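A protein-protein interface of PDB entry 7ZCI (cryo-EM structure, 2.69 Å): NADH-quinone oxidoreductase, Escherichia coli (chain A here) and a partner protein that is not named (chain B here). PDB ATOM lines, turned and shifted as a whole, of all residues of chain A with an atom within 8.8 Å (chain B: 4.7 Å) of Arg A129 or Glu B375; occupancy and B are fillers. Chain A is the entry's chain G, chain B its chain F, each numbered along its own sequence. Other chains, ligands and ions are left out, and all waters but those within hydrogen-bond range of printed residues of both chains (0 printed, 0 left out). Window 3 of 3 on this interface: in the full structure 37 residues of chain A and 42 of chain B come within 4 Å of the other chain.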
ATOM      1  N   GLU A  93      31.632 -30.317  29.878  1.00  0.00           N
ATOM      2  CA  GLU A  93      30.462 -29.477  29.632  1.00  0.00           C
ATOM      3  C   GLU A  93      30.662 -28.051  30.144  1.00  0.00           C
ATOM      4  O   GLU A  93      30.281 -27.081  29.475  1.00  0.00           O
ATOM      5  CB  GLU A  93      29.241 -30.114  30.290  1.00  0.00           C
ATOM      6  CG  GLU A  93      27.953 -29.369  30.059  1.00  0.00           C
ATOM      7  CD  GLU A  93      26.740 -30.174  30.457  1.00  0.00           C
ATOM      8  OE1 GLU A  93      26.783 -30.846  31.502  1.00  0.00           O
ATOM      9  OE2 GLU A  93      25.746 -30.148  29.712  1.00  0.00           O
ATOM     10  N   THR A  97      30.666 -24.517  27.921  1.00  0.00           N
ATOM     11  CA  THR A  97      29.637 -23.481  28.045  1.00  0.00           C
ATOM     12  C   THR A  97      30.069 -22.162  27.413  1.00  0.00           C
ATOM     13  O   THR A  97      29.259 -21.480  26.781  1.00  0.00           O
ATOM     14  CB  THR A  97      29.268 -23.240  29.511  1.00  0.00           C
ATOM     15  OG1 THR A  97      30.453 -23.024  30.280  1.00  0.00           O
ATOM     16  CG2 THR A  97      28.522 -24.417  30.078  1.00  0.00           C
ATOM     17  N   ARG A 126      24.641 -30.071  23.819  1.00  0.00           N
ATOM     18  CA  ARG A 126      24.677 -28.804  24.537  1.00  0.00           C
ATOM     19  C   ARG A 126      23.311 -28.544  25.153  1.00  0.00           C
ATOM     20  O   ARG A 126      22.312 -28.457  24.434  1.00  0.00           O
ATOM     21  CB  ARG A 126      25.063 -27.672  23.588  1.00  0.00           C
ATOM     22  CG  ARG A 126      25.337 -26.334  24.235  1.00  0.00           C
ATOM     23  CD  ARG A 126      25.936 -25.372  23.221  1.00  0.00           C
ATOM     24  NE  ARG A 126      26.217 -24.058  23.783  1.00  0.00           N
ATOM     25  CZ  ARG A 126      27.312 -23.743  24.460  1.00  0.00           C
ATOM     26  NH1 ARG A 126      28.254 -24.635  24.708  1.00  0.00           N
ATOM     27  NH2 ARG A 126      27.469 -22.498  24.893  1.00  0.00           N
ATOM     28  N   ARG A 127      23.266 -28.418  26.473  1.00  0.00           N
ATOM     29  CA  ARG A 127      22.058 -27.984  27.155  1.00  0.00           C
ATOM     30  C   ARG A 127      22.222 -26.624  27.807  1.00  0.00           C
ATOM     31  O   ARG A 127      21.300 -26.157  28.479  1.00  0.00           O
ATOM     32  CB  ARG A 127      21.622 -29.016  28.195  1.00  0.00           C
ATOM     33  CG  ARG A 127      22.633 -29.267  29.255  1.00  0.00           C
ATOM     34  CD  ARG A 127      22.467 -30.646  29.847  1.00  0.00           C
ATOM     35  NE  ARG A 127      23.398 -30.839  30.949  1.00  0.00           N
ATOM     36  CZ  ARG A 127      23.051 -30.862  32.227  1.00  0.00           C
ATOM     37  NH1 ARG A 127      21.787 -30.755  32.602  1.00  0.00           N
ATOM     38  NH2 ARG A 127      23.995 -30.992  33.152  1.00  0.00           N
ATOM     39  N   TYR A 128      23.373 -25.988  27.636  1.00  0.00           N
ATOM     40  CA  TYR A 128      23.568 -24.609  28.049  1.00  0.00           C
ATOM     41  C   TYR A 128      22.996 -23.679  26.989  1.00  0.00           C
ATOM     42  O   TYR A 128      23.310 -23.806  25.803  1.00  0.00           O
ATOM     43  CB  TYR A 128      25.056 -24.348  28.267  1.00  0.00           C
ATOM     44  CG  TYR A 128      25.426 -22.959  28.721  1.00  0.00           C
ATOM     45  CD1 TYR A 128      25.361 -22.601  30.055  1.00  0.00           C
ATOM     46  CD2 TYR A 128      25.880 -22.016  27.812  1.00  0.00           C
ATOM     47  CE1 TYR A 128      25.722 -21.343  30.464  1.00  0.00           C
ATOM     48  CE2 TYR A 128      26.238 -20.764  28.216  1.00  0.00           C
ATOM     49  CZ  TYR A 128      26.160 -20.429  29.538  1.00  0.00           C
ATOM     50  OH  TYR A 128      26.526 -19.167  29.919  1.00  0.00           O
ATOM     51  N   ARG A 129      22.150 -22.748  27.414  1.00  0.00           N
ATOM     52  CA  ARG A 129      21.430 -21.882  26.495  1.00  0.00           C
ATOM     53  C   ARG A 129      21.739 -20.405  26.677  1.00  0.00           C
ATOM     54  O   ARG A 129      21.173 -19.578  25.958  1.00  0.00           O
ATOM     55  CB  ARG A 129      19.922 -22.105  26.646  1.00  0.00           C
ATOM     56  CG  ARG A 129      19.339 -21.556  27.925  1.00  0.00           C
ATOM     57  CD  ARG A 129      17.836 -21.678  27.934  1.00  0.00           C
ATOM     58  NE  ARG A 129      17.251 -21.118  29.143  1.00  0.00           N
ATOM     59  CZ  ARG A 129      17.082 -21.789  30.271  1.00  0.00           C
ATOM     60  NH1 ARG A 129      17.449 -23.052  30.383  1.00  0.00           N
ATOM     61  NH2 ARG A 129      16.538 -21.174  31.315  1.00  0.00           N
ATOM     62  N   PHE A 130      22.614 -20.050  27.601  1.00  0.00           N
ATOM     63  CA  PHE A 130      22.906 -18.664  27.905  1.00  0.00           C
ATOM     64  C   PHE A 130      24.120 -18.194  27.113  1.00  0.00           C
ATOM     65  O   PHE A 130      24.602 -18.875  26.207  1.00  0.00           O
ATOM     66  CB  PHE A 130      23.084 -18.511  29.409  1.00  0.00           C
ATOM     67  CG  PHE A 130      21.998 -19.161  30.201  1.00  0.00           C
ATOM     68  CD1 PHE A 130      20.755 -18.570  30.305  1.00  0.00           C
ATOM     69  CD2 PHE A 130      22.210 -20.372  30.826  1.00  0.00           C
ATOM     70  CE1 PHE A 130      19.753 -19.171  31.024  1.00  0.00           C
ATOM     71  CE2 PHE A 130      21.209 -20.971  31.543  1.00  0.00           C
ATOM     72  CZ  PHE A 130      19.982 -20.371  31.644  1.00  0.00           C
ATOM     73  N   THR A 131      24.616 -17.008  27.446  1.00  0.00           N
ATOM     74  CA  THR A 131      25.643 -16.367  26.644  1.00  0.00           C
ATOM     75  C   THR A 131      27.032 -16.906  26.968  1.00  0.00           C
ATOM     76  O   THR A 131      27.295 -17.436  28.049  1.00  0.00           O
ATOM     77  CB  THR A 131      25.624 -14.853  26.848  1.00  0.00           C
ATOM     78  OG1 THR A 131      25.836 -14.551  28.231  1.00  0.00           O
ATOM     79  CG2 THR A 131      24.298 -14.278  26.412  1.00  0.00           C
ATOM     80  N   LYS A 132      27.929 -16.754  26.004  1.00  0.00           N
ATOM     81  CA  LYS A 132      29.330 -17.092  26.173  1.00  0.00           C
ATOM     82  C   LYS A 132      30.114 -15.824  26.455  1.00  0.00           C
ATOM     83  O   LYS A 132      29.885 -14.792  25.821  1.00  0.00           O
ATOM     84  CB  LYS A 132      29.898 -17.768  24.927  1.00  0.00           C
ATOM     85  CG  LYS A 132      29.126 -18.949  24.404  1.00  0.00           C
ATOM     86  CD  LYS A 132      29.679 -19.332  23.059  1.00  0.00           C
ATOM     87  CE  LYS A 132      29.098 -20.613  22.530  1.00  0.00           C
ATOM     88  NZ  LYS A 132      29.636 -20.875  21.175  1.00  0.00           N
ATOM     89  N   ALA B 370      17.071 -16.669  35.217  1.00  0.00           N
ATOM     90  CA  ALA B 370      15.950 -17.069  34.375  1.00  0.00           C
ATOM     91  C   ALA B 370      14.729 -17.442  35.210  1.00  0.00           C
ATOM     92  O   ALA B 370      13.601 -17.079  34.863  1.00  0.00           O
ATOM     93  CB  ALA B 370      16.362 -18.231  33.474  1.00  0.00           C
ATOM     94  N   ARG B 373      13.179 -14.229  36.651  1.00  0.00           N
ATOM     95  CA  ARG B 373      12.407 -13.496  35.657  1.00  0.00           C
ATOM     96  C   ARG B 373      11.218 -14.285  35.129  1.00  0.00           C
ATOM     97  O   ARG B 373      10.474 -13.764  34.293  1.00  0.00           O
ATOM     98  CB  ARG B 373      13.298 -13.090  34.483  1.00  0.00           C
ATOM     99  CG  ARG B 373      14.373 -12.091  34.836  1.00  0.00           C
ATOM    100  CD  ARG B 373      15.133 -11.656  33.603  1.00  0.00           C
ATOM    101  NE  ARG B 373      15.253 -12.737  32.633  1.00  0.00           N
ATOM    102  CZ  ARG B 373      16.333 -13.493  32.485  1.00  0.00           C
ATOM    103  NH1 ARG B 373      17.412 -13.312  33.230  1.00  0.00           N
ATOM    104  NH2 ARG B 373      16.330 -14.452  31.565  1.00  0.00           N
ATOM    105  N   GLY B 374      11.024 -15.518  35.581  1.00  0.00           N
ATOM    106  CA  GLY B 374       9.972 -16.351  35.051  1.00  0.00           C
ATOM    107  C   GLY B 374      10.269 -16.986  33.714  1.00  0.00           C
ATOM    108  O   GLY B 374       9.359 -17.544  33.098  1.00  0.00           O
ATOM    109  N   GLU B 375      11.513 -16.924  33.239  1.00  0.00           N
ATOM    110  CA  GLU B 375      11.897 -17.511  31.964  1.00  0.00           C
ATOM    111  C   GLU B 375      12.577 -18.864  32.129  1.00  0.00           C
ATOM    112  O   GLU B 375      13.402 -19.250  31.296  1.00  0.00           O
ATOM    113  CB  GLU B 375      12.803 -16.554  31.196  1.00  0.00           C
ATOM    114  CG  GLU B 375      12.272 -15.141  31.117  1.00  0.00           C
ATOM    115  CD  GLU B 375      13.203 -14.212  30.373  1.00  0.00           C
ATOM    116  OE1 GLU B 375      13.616 -14.562  29.248  1.00  0.00           O
ATOM    117  OE2 GLU B 375      13.528 -13.135  30.913  1.00  0.00           O
ATOM    118  N   GLY B 376      12.256 -19.588  33.195  1.00  0.00           N
ATOM    119  CA  GLY B 376      12.834 -20.901  33.387  1.00  0.00           C
ATOM    120  C   GLY B 376      12.317 -21.904  32.375  1.00  0.00           C
ATOM    121  O   GLY B 376      11.232 -21.764  31.817  1.00  0.00           O
ATOM    122  N   GLN B 377      13.121 -22.928  32.133  1.00  0.00           N
ATOM    123  CA  GLN B 377      12.820 -23.967  31.165  1.00  0.00           C
ATOM    124  C   GLN B 377      13.028 -25.321  31.822  1.00  0.00           C
ATOM    125  O   GLN B 377      13.784 -25.420  32.790  1.00  0.00           O
ATOM    126  CB  GLN B 377      13.712 -23.823  29.924  1.00  0.00           C
ATOM    127  CG  GLN B 377      13.419 -22.564  29.129  1.00  0.00           C
ATOM    128  CD  GLN B 377      14.273 -22.431  27.893  1.00  0.00           C
ATOM    129  OE1 GLN B 377      14.978 -23.357  27.511  1.00  0.00           O
ATOM    130  NE2 GLN B 377      14.220 -21.268  27.265  1.00  0.00           N
ATOM    131  N   ASP B 380      16.006 -27.176  34.288  1.00  0.00           N
ATOM    132  CA  ASP B 380      16.780 -26.197  35.044  1.00  0.00           C
ATOM    133  C   ASP B 380      16.993 -26.640  36.485  1.00  0.00           C
ATOM    134  O   ASP B 380      18.094 -26.491  37.024  1.00  0.00           O
ATOM    135  CB  ASP B 380      16.088 -24.837  35.003  1.00  0.00           C
ATOM    136  CG  ASP B 380      16.459 -24.032  33.779  1.00  0.00           C
ATOM    137  OD1 ASP B 380      17.271 -24.519  32.969  1.00  0.00           O
ATOM    138  OD2 ASP B 380      15.926 -22.921  33.612  1.00  0.00           O
ATOM    139  N   GLY B 422       9.269 -20.865  38.841  1.00  0.00           N
ATOM    140  CA  GLY B 422      10.071 -20.123  37.884  1.00  0.00           C
ATOM    141  C   GLY B 422      10.007 -20.640  36.457  1.00  0.00           C
ATOM    142  O   GLY B 422      10.296 -19.886  35.526  1.00  0.00           O
ATOM    143  N   GLN B 425       8.709 -21.453  30.317  1.00  0.00           N
ATOM    144  CA  GLN B 425       8.946 -21.544  28.884  1.00  0.00           C
ATOM    145  C   GLN B 425       9.323 -22.968  28.488  1.00  0.00           C
ATOM    146  O   GLN B 425       9.864 -23.713  29.306  1.00  0.00           O
ATOM    147  CB  GLN B 425      10.068 -20.590  28.459  1.00  0.00           C
ATOM    148  CG  GLN B 425       9.749 -19.135  28.697  1.00  0.00           C
ATOM    149  CD  GLN B 425      10.838 -18.212  28.202  1.00  0.00           C
ATOM    150  OE1 GLN B 425      11.957 -18.640  27.926  1.00  0.00           O
ATOM    151  NE2 GLN B 425      10.514 -16.931  28.086  1.00  0.00           N
ATOM    152  N   PHE B 427      11.658 -25.824  26.699  1.00  0.00           N
ATOM    153  CA  PHE B 427      13.109 -25.876  26.582  1.00  0.00           C
ATOM    154  C   PHE B 427      13.545 -25.698  25.136  1.00  0.00           C
ATOM    155  O   PHE B 427      13.038 -26.369  24.234  1.00  0.00           O
ATOM    156  CB  PHE B 427      13.676 -27.185  27.123  1.00  0.00           C
ATOM    157  CG  PHE B 427      15.151 -27.319  26.889  1.00  0.00           C
ATOM    158  CD1 PHE B 427      16.043 -26.510  27.571  1.00  0.00           C
ATOM    159  CD2 PHE B 427      15.646 -28.209  25.952  1.00  0.00           C
ATOM    160  CE1 PHE B 427      17.396 -26.600  27.344  1.00  0.00           C
ATOM    161  CE2 PHE B 427      17.000 -28.302  25.721  1.00  0.00           C
ATOM    162  CZ  PHE B 427      17.875 -27.498  26.421  1.00  0.00           C
ATOM    163  N   SER B 428      14.517 -24.814  24.928  1.00  0.00           N
ATOM    164  CA  SER B 428      15.049 -24.553  23.598  1.00  0.00           C
ATOM    165  C   SER B 428      16.413 -23.898  23.731  1.00  0.00           C
ATOM    166  O   SER B 428      16.571 -22.949  24.501  1.00  0.00           O
ATOM    167  CB  SER B 428      14.107 -23.653  22.793  1.00  0.00           C
ATOM    168  OG  SER B 428      14.623 -23.393  21.500  1.00  0.00           O
ATOM    169  N   ASN B 429      17.393 -24.416  22.990  1.00  0.00           N
ATOM    170  CA  ASN B 429      18.662 -23.728  22.781  1.00  0.00           C
ATOM    171  C   ASN B 429      19.089 -23.811  21.323  1.00  0.00           C
ATOM    172  O   ASN B 429      20.234 -23.498  20.997  1.00  0.00           O
ATOM    173  CB  ASN B 429      19.757 -24.272  23.704  1.00  0.00           C
ATOM    174  CG  ASN B 429      20.059 -25.732  23.472  1.00  0.00           C
ATOM    175  OD1 ASN B 429      19.255 -26.468  22.910  1.00  0.00           O
ATOM    176  ND2 ASN B 429      21.218 -26.168  23.940  1.00  0.00           N
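OD2 of Asp B380 is in salt-bridge range of NH2 of Arg A129 (3.0 Å).
O of Arg A126 lies within hydrogen-bond range of ND2 of Asn B429 (2.6 Å).
N of Glu B375 lies within hydrogen-bond range of O of Ala B370 (2.6 Å).
N of Gly B376 is in hydrogen-bond range of O of Ala B370.
The backbone NH (N) of Ser B428 sits at hydrogen-bond distance from the side-chain amide oxygen (OE1) of Gln B377, 3.0 Å away.
The backbone NH (N) of Gln B377 lies within hydrogen-bond range of the side-chain carboxylate (OD2) of Asp B380 (3.2 Å).
The guanidinium group (NE) of Arg B373 lies within salt-bridge range of the side-chain carboxylate (OE2) of Glu B375, 2.5 Å away.
The side-chain carboxylate of Glu A93 lies within salt-bridge range of the guanidinium group of Arg A127 (2.7 Å).
Among the printed residues, pairs that only touch across the chains: Arg A127 with Asn B429, Tyr A128 with Asn B429, Arg A129 with Ala B370, Arg A129 with Glu B375, Arg A129 with Gln B377, Arg A129 with Ser B428 and Arg A129 with Asn B429.
Glu B375 touches just one residue of chain A: Arg A129 (3.7 Å).
No residue of chain A comes within 4 Å of Arg B373.
No residue of chain A comes within 4 Å of Gly B374.
No residue of chain A comes within 4 Å of Gly B376.
Printed residues of chain B within 4 Å of Arg A127: Asn B429 (3.8 Å).
Of the printed residues of chain B, Arg A126 touches Asn B429.
Lys A132 touches none of the printed residues of chain B.
The nearest residue of chain A that does not touch Glu B375 is Phe A130 (6.4 Å).
Of the 12 printed residues of chain B, 6 touch a printed residue of chain A.
Printed residues of chain B that touch a printed residue of chain A: Ala B370, Glu B375, Gln B377, Asp B380, Ser B428 and Asn B429.
Along chain A the printed residues that touch a printed residue of chain B span positions 126 to 129.
Among the printed residues, Asp or Glu carboxylates within 4 Å of a Lys or Arg side-chain nitrogen of the other chain: Arg A129 with Asp B380 (3.0 Å).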
